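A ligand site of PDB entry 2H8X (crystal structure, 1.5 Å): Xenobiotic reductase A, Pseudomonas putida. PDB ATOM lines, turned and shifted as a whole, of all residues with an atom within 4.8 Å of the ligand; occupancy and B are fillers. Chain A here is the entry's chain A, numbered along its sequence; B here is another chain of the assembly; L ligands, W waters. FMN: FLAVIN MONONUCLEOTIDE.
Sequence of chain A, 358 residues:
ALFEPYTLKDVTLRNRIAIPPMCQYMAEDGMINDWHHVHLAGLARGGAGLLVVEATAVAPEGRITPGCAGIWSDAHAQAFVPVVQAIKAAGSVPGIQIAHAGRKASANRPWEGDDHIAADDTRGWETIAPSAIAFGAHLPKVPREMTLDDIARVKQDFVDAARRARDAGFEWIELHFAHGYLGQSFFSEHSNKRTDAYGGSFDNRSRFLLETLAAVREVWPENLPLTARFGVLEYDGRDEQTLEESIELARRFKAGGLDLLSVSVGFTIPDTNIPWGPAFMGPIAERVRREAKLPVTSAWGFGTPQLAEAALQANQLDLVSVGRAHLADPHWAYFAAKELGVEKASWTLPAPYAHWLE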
ATOM      1  N   PRO A  20      23.198  17.021 -30.040  1.00  0.00           N
ATOM      2  CA  PRO A  20      24.346  17.831 -29.634  1.00  0.00           C
ATOM      3  C   PRO A  20      25.563  16.990 -29.326  1.00  0.00           C
ATOM      4  O   PRO A  20      25.466  15.777 -29.092  1.00  0.00           O
ATOM      5  CB  PRO A  20      23.824  18.575 -28.421  1.00  0.00           C
ATOM      6  CG  PRO A  20      22.969  17.532 -27.751  1.00  0.00           C
ATOM      7  CD  PRO A  20      22.212  16.914 -28.936  1.00  0.00           C
ATOM      8  N   PRO A  21      26.751  17.611 -29.328  1.00  0.00           N
ATOM      9  CA  PRO A  21      27.968  16.850 -29.033  1.00  0.00           C
ATOM     10  C   PRO A  21      27.880  16.246 -27.640  1.00  0.00           C
ATOM     11  O   PRO A  21      27.495  16.922 -26.685  1.00  0.00           O
ATOM     12  CB  PRO A  21      29.073  17.893 -29.153  1.00  0.00           C
ATOM     13  CG  PRO A  21      28.372  19.177 -28.818  1.00  0.00           C
ATOM     14  CD  PRO A  21      27.072  19.040 -29.560  1.00  0.00           C
ATOM     15  N   MET A  22      28.226  14.966 -27.535  1.00  0.00           N
ATOM     16  CA  MET A  22      28.215  14.282 -26.258  1.00  0.00           C
ATOM     17  C   MET A  22      29.436  13.372 -26.092  1.00  0.00           C
ATOM     18  O   MET A  22      29.507  12.297 -26.665  1.00  0.00           O
ATOM     19  CB  MET A  22      26.930  13.465 -26.077  1.00  0.00           C
ATOM     20  CG  MET A  22      25.683  14.310 -25.805  1.00  0.00           C
ATOM     21  SD  MET A  22      24.210  13.289 -25.473  1.00  0.00           S
ATOM     22  CE  MET A  22      23.827  12.730 -27.132  1.00  0.00           C
ATOM     23  N   CYS A  23      30.400  13.834 -25.290  1.00  0.00           N
ATOM     24  CA  CYS A  23      31.609  13.083 -25.012  1.00  0.00           C
ATOM     25  C   CYS A  23      31.289  11.657 -24.583  1.00  0.00           C
ATOM     26  O   CYS A  23      30.359  11.420 -23.804  1.00  0.00           O
ATOM     27  CB  CYS A  23      32.425  13.751 -23.911  1.00  0.00           C
ATOM     28  SG  CYS A  23      33.383  15.181 -24.436  1.00  0.00           S
ATOM     29  N   TYR A  25      34.170   9.506 -23.860  1.00  0.00           N
ATOM     30  CA  TYR A  25      35.328   9.125 -23.052  1.00  0.00           C
ATOM     31  C   TYR A  25      35.815   7.717 -23.372  1.00  0.00           C
ATOM     32  O   TYR A  25      36.339   7.021 -22.490  1.00  0.00           O
ATOM     33  CB  TYR A  25      34.967   9.217 -21.556  1.00  0.00           C
ATOM     34  CG  TYR A  25      34.310  10.530 -21.179  1.00  0.00           C
ATOM     35  CD1 TYR A  25      35.079  11.663 -20.884  1.00  0.00           C
ATOM     36  CD2 TYR A  25      32.921  10.654 -21.154  1.00  0.00           C
ATOM     37  CE1 TYR A  25      34.473  12.878 -20.561  1.00  0.00           C
ATOM     38  CE2 TYR A  25      32.308  11.859 -20.838  1.00  0.00           C
ATOM     39  CZ  TYR A  25      33.095  12.969 -20.542  1.00  0.00           C
ATOM     40  OH  TYR A  25      32.485  14.164 -20.216  1.00  0.00           O
ATOM     41  N   GLU A  54      30.993  14.496 -30.632  1.00  0.00           N
ATOM     42  CA  GLU A  54      31.493  14.999 -29.349  1.00  0.00           C
ATOM     43  C   GLU A  54      32.715  15.908 -29.456  1.00  0.00           C
ATOM     44  O   GLU A  54      33.425  15.894 -30.451  1.00  0.00           O
ATOM     45  CB  GLU A  54      31.869  13.818 -28.467  1.00  0.00           C
ATOM     46  CG  GLU A  54      32.989  12.987 -29.072  1.00  0.00           C
ATOM     47  CD  GLU A  54      33.132  11.648 -28.410  1.00  0.00           C
ATOM     48  OE1 GLU A  54      33.769  11.567 -27.345  1.00  0.00           O
ATOM     49  OE2 GLU A  54      32.598  10.667 -28.954  1.00  0.00           O
ATOM     50  N   ALA A  55      32.950  16.680 -28.388  1.00  0.00           N
ATOM     51  CA  ALA A  55      34.097  17.571 -28.334  1.00  0.00           C
ATOM     52  C   ALA A  55      35.352  16.805 -28.705  1.00  0.00           C
ATOM     53  O   ALA A  55      35.755  15.862 -28.017  1.00  0.00           O
ATOM     54  CB  ALA A  55      34.247  18.153 -26.931  1.00  0.00           C
ATOM     55  N   GLN A  97      32.196  18.888 -33.228  1.00  0.00           N
ATOM     56  CA  GLN A  97      32.568  20.007 -32.376  1.00  0.00           C
ATOM     57  C   GLN A  97      34.064  19.890 -32.092  1.00  0.00           C
ATOM     58  O   GLN A  97      34.521  18.886 -31.565  1.00  0.00           O
ATOM     59  CB  GLN A  97      31.798  19.939 -31.052  1.00  0.00           C
ATOM     60  CG  GLN A  97      32.115  21.090 -30.107  1.00  0.00           C
ATOM     61  CD  GLN A  97      31.540  20.871 -28.713  1.00  0.00           C
ATOM     62  OE1 GLN A  97      31.911  19.925 -28.018  1.00  0.00           O
ATOM     63  NE2 GLN A  97      30.649  21.759 -28.307  1.00  0.00           N
ATOM     64  N   GLU A 174      31.310  22.966 -35.405  1.00  0.00           N
ATOM     65  CA  GLU A 174      30.955  23.765 -34.236  1.00  0.00           C
ATOM     66  C   GLU A 174      32.186  24.031 -33.384  1.00  0.00           C
ATOM     67  O   GLU A 174      32.829  23.089 -32.913  1.00  0.00           O
ATOM     68  CB  GLU A 174      29.892  23.047 -33.395  1.00  0.00           C
ATOM     69  CG  GLU A 174      29.430  23.833 -32.160  1.00  0.00           C
ATOM     70  CD  GLU A 174      28.502  23.037 -31.261  1.00  0.00           C
ATOM     71  OE1 GLU A 174      27.387  22.698 -31.691  1.00  0.00           O
ATOM     72  OE2 GLU A 174      28.891  22.746 -30.102  1.00  0.00           O
ATOM     73  N   HIS A 176      33.881  24.952 -30.033  1.00  0.00           N
ATOM     74  CA  HIS A 176      33.473  24.867 -28.636  1.00  0.00           C
ATOM     75  C   HIS A 176      33.988  26.012 -27.777  1.00  0.00           C
ATOM     76  O   HIS A 176      35.041  25.906 -27.141  1.00  0.00           O
ATOM     77  CB  HIS A 176      33.944  23.531 -28.045  1.00  0.00           C
ATOM     78  CG  HIS A 176      33.228  23.149 -26.775  1.00  0.00           C
ATOM     79  ND1 HIS A 176      32.419  24.025 -26.091  1.00  0.00           N
ATOM     80  CD2 HIS A 176      33.194  21.978 -26.100  1.00  0.00           C
ATOM     81  CE1 HIS A 176      31.906  23.406 -25.036  1.00  0.00           C
ATOM     82  NE2 HIS A 176      32.363  22.167 -25.022  1.00  0.00           N
ATOM     83  N   HIS A 179      31.102  26.240 -21.854  1.00  0.00           N
ATOM     84  CA  HIS A 179      31.326  25.374 -20.706  1.00  0.00           C
ATOM     85  C   HIS A 179      32.626  25.526 -19.930  1.00  0.00           C
ATOM     86  O   HIS A 179      33.141  24.548 -19.358  1.00  0.00           O
ATOM     87  CB  HIS A 179      31.088  23.930 -21.158  1.00  0.00           C
ATOM     88  CG  HIS A 179      29.742  23.723 -21.789  1.00  0.00           C
ATOM     89  ND1 HIS A 179      29.422  22.589 -22.509  1.00  0.00           N
ATOM     90  CD2 HIS A 179      28.636  24.499 -21.789  1.00  0.00           C
ATOM     91  CE1 HIS A 179      28.173  22.686 -22.932  1.00  0.00           C
ATOM     92  NE2 HIS A 179      27.679  23.830 -22.512  1.00  0.00           N
ATOM     93  N   ARG A 229      29.456  27.002 -30.119  1.00  0.00           N
ATOM     94  CA  ARG A 229      28.653  26.905 -28.915  1.00  0.00           C
ATOM     95  C   ARG A 229      29.292  27.924 -27.978  1.00  0.00           C
ATOM     96  O   ARG A 229      30.511  28.046 -27.914  1.00  0.00           O
ATOM     97  CB  ARG A 229      28.679  25.500 -28.299  1.00  0.00           C
ATOM     98  CG  ARG A 229      27.331  25.123 -27.697  1.00  0.00           C
ATOM     99  CD  ARG A 229      27.418  24.599 -26.305  1.00  0.00           C
ATOM    100  NE  ARG A 229      27.374  23.139 -26.255  1.00  0.00           N
ATOM    101  CZ  ARG A 229      26.258  22.402 -26.165  1.00  0.00           C
ATOM    102  NH1 ARG A 229      25.056  22.947 -26.106  1.00  0.00           N
ATOM    103  NH2 ARG A 229      26.377  21.090 -26.086  1.00  0.00           N
ATOM    104  N   ALA A 299      19.759  23.443 -25.554  1.00  0.00           N
ATOM    105  CA  ALA A 299      19.445  22.131 -25.024  1.00  0.00           C
ATOM    106  C   ALA A 299      19.095  22.178 -23.547  1.00  0.00           C
ATOM    107  O   ALA A 299      19.152  23.227 -22.911  1.00  0.00           O
ATOM    108  CB  ALA A 299      20.619  21.193 -25.239  1.00  0.00           C
ATOM    109  N   TRP A 300      18.744  20.991 -23.053  1.00  0.00           N
ATOM    110  CA  TRP A 300      18.372  20.694 -21.665  1.00  0.00           C
ATOM    111  C   TRP A 300      16.888  20.491 -21.439  1.00  0.00           C
ATOM    112  O   TRP A 300      16.142  21.451 -21.239  1.00  0.00           O
ATOM    113  CB  TRP A 300      18.883  21.743 -20.674  1.00  0.00           C
ATOM    114  CG  TRP A 300      18.681  21.295 -19.259  1.00  0.00           C
ATOM    115  CD1 TRP A 300      17.528  21.359 -18.523  1.00  0.00           C
ATOM    116  CD2 TRP A 300      19.635  20.604 -18.441  1.00  0.00           C
ATOM    117  NE1 TRP A 300      17.706  20.757 -17.303  1.00  0.00           N
ATOM    118  CE2 TRP A 300      18.995  20.284 -17.229  1.00  0.00           C
ATOM    119  CE3 TRP A 300      20.975  20.234 -18.622  1.00  0.00           C
ATOM    120  CZ2 TRP A 300      19.636  19.594 -16.197  1.00  0.00           C
ATOM    121  CZ3 TRP A 300      21.613  19.554 -17.599  1.00  0.00           C
ATOM    122  CH2 TRP A 300      20.954  19.236 -16.399  1.00  0.00           C
ATOM    123  N   GLY A 301      16.475  19.233 -21.470  1.00  0.00           N
ATOM    124  CA  GLY A 301      15.085  18.892 -21.229  1.00  0.00           C
ATOM    125  C   GLY A 301      14.171  18.843 -22.440  1.00  0.00           C
ATOM    126  O   GLY A 301      12.956  18.736 -22.285  1.00  0.00           O
ATOM    127  N   PHE A 302      14.730  18.903 -23.636  1.00  0.00           N
ATOM    128  CA  PHE A 302      13.900  18.861 -24.828  1.00  0.00           C
ATOM    129  C   PHE A 302      13.555  17.448 -25.273  1.00  0.00           C
ATOM    130  O   PHE A 302      12.963  17.244 -26.339  1.00  0.00           O
ATOM    131  CB  PHE A 302      14.555  19.659 -25.960  1.00  0.00           C
ATOM    132  CG  PHE A 302      14.506  21.148 -25.743  1.00  0.00           C
ATOM    133  CD1 PHE A 302      13.318  21.848 -25.904  1.00  0.00           C
ATOM    134  CD2 PHE A 302      15.653  21.835 -25.347  1.00  0.00           C
ATOM    135  CE1 PHE A 302      13.266  23.225 -25.685  1.00  0.00           C
ATOM    136  CE2 PHE A 302      15.605  23.212 -25.119  1.00  0.00           C
ATOM    137  CZ  PHE A 302      14.411  23.903 -25.287  1.00  0.00           C
ATOM    138  N   SER A 321      18.116  20.762 -29.753  1.00  0.00           N
ATOM    139  CA  SER A 321      19.156  19.793 -29.406  1.00  0.00           C
ATOM    140  C   SER A 321      18.646  18.861 -28.315  1.00  0.00           C
ATOM    141  O   SER A 321      18.202  19.315 -27.264  1.00  0.00           O
ATOM    142  CB  SER A 321      20.412  20.512 -28.924  1.00  0.00           C
ATOM    143  OG  SER A 321      20.991  21.271 -29.986  1.00  0.00           O
ATOM    144  N   VAL A 322      18.714  17.558 -28.579  1.00  0.00           N
ATOM    145  CA  VAL A 322      18.245  16.527 -27.653  1.00  0.00           C
ATOM    146  C   VAL A 322      19.417  15.599 -27.363  1.00  0.00           C
ATOM    147  O   VAL A 322      19.836  14.826 -28.220  1.00  0.00           O
ATOM    148  CB  VAL A 322      17.092  15.730 -28.290  1.00  0.00           C
ATOM    149  CG1 VAL A 322      16.548  14.689 -27.306  1.00  0.00           C
ATOM    150  CG2 VAL A 322      15.974  16.682 -28.718  1.00  0.00           C
ATOM    151  N   GLY A 323      19.942  15.681 -26.138  1.00  0.00           N
ATOM    152  CA  GLY A 323      21.092  14.879 -25.778  1.00  0.00           C
ATOM    153  C   GLY A 323      20.875  13.558 -25.084  1.00  0.00           C
ATOM    154  O   GLY A 323      20.849  12.503 -25.727  1.00  0.00           O
ATOM    155  N   ARG A 324      20.714  13.603 -23.769  1.00  0.00           N
ATOM    156  CA  ARG A 324      20.542  12.387 -22.986  1.00  0.00           C
ATOM    157  C   ARG A 324      19.429  11.442 -23.436  1.00  0.00           C
ATOM    158  O   ARG A 324      19.561  10.234 -23.319  1.00  0.00           O
ATOM    159  CB  ARG A 324      20.384  12.738 -21.500  1.00  0.00           C
ATOM    160  CG  ARG A 324      21.723  13.142 -20.866  1.00  0.00           C
ATOM    161  CD  ARG A 324      21.558  13.766 -19.507  1.00  0.00           C
ATOM    162  NE  ARG A 324      20.867  15.050 -19.589  1.00  0.00           N
ATOM    163  CZ  ARG A 324      20.600  15.828 -18.543  1.00  0.00           C
ATOM    164  NH1 ARG A 324      20.962  15.447 -17.332  1.00  0.00           N
ATOM    165  NH2 ARG A 324      19.958  16.979 -18.724  1.00  0.00           N
ATOM    166  N   LEU A 327      20.779   8.936 -25.618  1.00  0.00           N
ATOM    167  CA  LEU A 327      21.640   7.938 -25.022  1.00  0.00           C
ATOM    168  C   LEU A 327      20.699   6.841 -24.510  1.00  0.00           C
ATOM    169  O   LEU A 327      21.006   5.648 -24.605  1.00  0.00           O
ATOM    170  CB  LEU A 327      22.450   8.533 -23.858  1.00  0.00           C
ATOM    171  CG  LEU A 327      23.355   9.718 -24.208  1.00  0.00           C
ATOM    172  CD1 LEU A 327      24.125  10.165 -22.971  1.00  0.00           C
ATOM    173  CD2 LEU A 327      24.328   9.326 -25.301  1.00  0.00           C
ATOM    174  N   PRO B 352      29.364   4.858 -20.719  1.00  0.00           N
ATOM    175  CA  PRO B 352      29.169   6.116 -21.453  1.00  0.00           C
ATOM    176  C   PRO B 352      27.716   6.589 -21.521  1.00  0.00           C
ATOM    177  O   PRO B 352      27.464   7.759 -21.799  1.00  0.00           O
ATOM    178  CB  PRO B 352      29.734   5.805 -22.837  1.00  0.00           C
ATOM    179  CG  PRO B 352      30.833   4.822 -22.526  1.00  0.00           C
ATOM    180  CD  PRO B 352      30.164   3.908 -21.525  1.00  0.00           C
ATOM    181  N   TRP B 356      25.080   8.895 -17.091  1.00  0.00           N
ATOM    182  CA  TRP B 356      24.216  10.068 -17.254  1.00  0.00           C
ATOM    183  C   TRP B 356      22.721   9.837 -17.114  1.00  0.00           C
ATOM    184  O   TRP B 356      21.958  10.797 -17.021  1.00  0.00           O
ATOM    185  CB  TRP B 356      24.498  10.693 -18.613  1.00  0.00           C
ATOM    186  CG  TRP B 356      25.948  10.797 -18.853  1.00  0.00           C
ATOM    187  CD1 TRP B 356      26.738   9.916 -19.526  1.00  0.00           C
ATOM    188  CD2 TRP B 356      26.818  11.798 -18.314  1.00  0.00           C
ATOM    189  NE1 TRP B 356      28.059  10.298 -19.444  1.00  0.00           N
ATOM    190  CE2 TRP B 356      28.135  11.458 -18.704  1.00  0.00           C
ATOM    191  CE3 TRP B 356      26.620  12.950 -17.548  1.00  0.00           C
ATOM    192  CZ2 TRP B 356      29.244  12.219 -18.343  1.00  0.00           C
ATOM    193  CZ3 TRP B 356      27.715  13.713 -17.191  1.00  0.00           C
ATOM    194  CH2 TRP B 356      29.017  13.344 -17.594  1.00  0.00           C
HETATM  195  N1  FMN L   1      28.360  19.736 -24.613  1.00  0.00           N
HETATM  196  C2  FMN L   1      29.333  20.237 -25.432  1.00  0.00           C
HETATM  197  O2  FMN L   1      29.333  21.279 -25.792  1.00  0.00           O
HETATM  198  N3  FMN L   1      30.416  19.304 -25.838  1.00  0.00           N
HETATM  199  C4  FMN L   1      30.522  17.942 -25.423  1.00  0.00           C
HETATM  200  O4  FMN L   1      31.443  17.195 -25.801  1.00  0.00           O
HETATM  201  C4A FMN L   1      29.476  17.411 -24.535  1.00  0.00           C
HETATM  202  N5  FMN L   1      29.482  16.112 -24.094  1.00  0.00           N
HETATM  203  C5A FMN L   1      28.452  15.592 -23.264  1.00  0.00           C
HETATM  204  C6  FMN L   1      28.566  14.121 -22.888  1.00  0.00           C
HETATM  205  C7  FMN L   1      27.529  13.570 -22.076  1.00  0.00           C
HETATM  206  C7M FMN L   1      27.754  12.198 -21.815  1.00  0.00           C
HETATM  207  C8  FMN L   1      26.260  14.419 -21.545  1.00  0.00           C
HETATM  208  C8M FMN L   1      25.188  13.983 -20.759  1.00  0.00           C
HETATM  209  C9  FMN L   1      26.234  15.759 -21.938  1.00  0.00           C
HETATM  210  C9A FMN L   1      27.279  16.445 -22.814  1.00  0.00           C
HETATM  211  N10 FMN L   1      27.331  17.909 -23.327  1.00  0.00           N
HETATM  212  C10 FMN L   1      28.368  18.446 -24.174  1.00  0.00           C
HETATM  213  C1' FMN L   1      26.191  18.724 -22.886  1.00  0.00           C
HETATM  214  C2' FMN L   1      25.035  18.255 -24.039  1.00  0.00           C
HETATM  215  O2' FMN L   1      25.430  18.613 -25.395  1.00  0.00           O
HETATM  216  C3' FMN L   1      23.658  18.878 -23.850  1.00  0.00           C
HETATM  217  O3' FMN L   1      23.717  20.342 -24.016  1.00  0.00           O
HETATM  218  C4' FMN L   1      23.156  18.506 -22.429  1.00  0.00           C
HETATM  219  O4' FMN L   1      23.112  17.072 -22.249  1.00  0.00           O
HETATM  220  C5' FMN L   1      21.770  19.051 -22.140  1.00  0.00           C
HETATM  221  O5' FMN L   1      20.741  18.413 -23.053  1.00  0.00           O
HETATM  222  P   FMN L   1      19.850  17.154 -22.629  1.00  0.00           P
HETATM  223  O1P FMN L   1      20.698  16.003 -22.304  1.00  0.00           O
HETATM  224  O2P FMN L   1      18.987  17.587 -21.451  1.00  0.00           O
HETATM  225  O3P FMN L   1      18.991  16.907 -23.860  1.00  0.00           O
HETATM  226  O   HOH W   1      17.605  18.985 -24.615  1.00  0.00           O
HETATM  227  O   HOH W   2      29.699   9.481 -21.863  1.00  0.00           O
HETATM  228  O   HOH W   3      27.328  20.508 -20.443  1.00  0.00           O
HETATM  229  O   HOH W   4      17.324  14.655 -23.762  1.00  0.00           O
HETATM  230  O   HOH W   5      26.163  18.074 -19.479  1.00  0.00           O
HETATM  231  O   HOH W   6      23.773  16.955 -19.314  1.00  0.00           O
HETATM  232  O   HOH W   7      17.239  15.895 -20.302  1.00  0.00           O
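The side-chain amide oxygen (OE1) of Gln 97 sits at hydrogen-bond distance from a nitrogen (N3) of the ligand (2.7 Å). The backbone NH (N) of Ala 55 is in hydrogen-bond range of an oxygen (O4) of the ligand (3.0 Å). NE2 of His 176 is in hydrogen-bond range of O2 of the ligand (3.2 Å). The backbone carbonyl oxygen of Pro 21 sits close to an oxygen (O2') of the ligand, 3.0 Å away. NH2 of Arg 229 is in hydrogen-bond range of O2' of the ligand (2.7 Å). O4 of the ligand is in hydrogen-bond range of SG of Cys 23, 3.1 Å away. N5 of the ligand lies within hydrogen-bond range of N of Cys 23. N of Trp 300 lies within hydrogen-bond range of O5' of the ligand (3.3 Å). N of Gly 323 is in hydrogen-bond range of O3P of the ligand (2.8 Å). An oxygen (O2P) of the ligand lies within hydrogen-bond range of the backbone NH (N) of Gly 301 (3.0 Å). NE of Arg 324 lies within salt-bridge range of O1P of the ligand, at 2.9 Å. The backbone NH (N) of Arg 324 is in hydrogen-bond range of an oxygen (O1P) of the ligand (2.8 Å).
Water W7 bridges O2P of the ligand (2.7 Å) and NH2 of Arg 324 (3.3 Å). Water W6 lies within hydrogen-bond range of an oxygen (O4') of the ligand (3.0 Å) and the guanidinium group of Arg 324 (3.5 Å). Water W2 lies within hydrogen-bond range of the backbone carbonyl oxygen of Cys 23, the backbone carbonyl oxygen of Pro 352 of chain B and the indole nitrogen of Trp 356 of chain B.
The side-chain amide nitrogen of Gln 97 lies within hydrogen-bond range of the side-chain carboxylate of Glu 174. OE1 of Gln 97 lies close to N of Ala 55, at 3.4 Å.
Pro 20 touches the ligand. Met 22 touches the ligand (CA to N5, 3.1 Å). CE1 of His 179 touches O2 of the ligand, 3.4 Å away. Ala 299 touches the ligand (CB to O3', 3.4 Å). C of Val 322 touches O3P of the ligand (3.8 Å). Trp 356 of chain B touches the ligand. Hydrophobic or aromatic side chains within 4 Å of the ligand: Pro 20, Pro 21, Met 22, Ala 55, His 176, His 179, Ala 299, Trp 300 and Trp 356 of chain B. Of the 23 residues printed, 16 come within 4 Å of the ligand. The nearest printed residue that does not touch the ligand is Glu 54 (4.1 Å).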
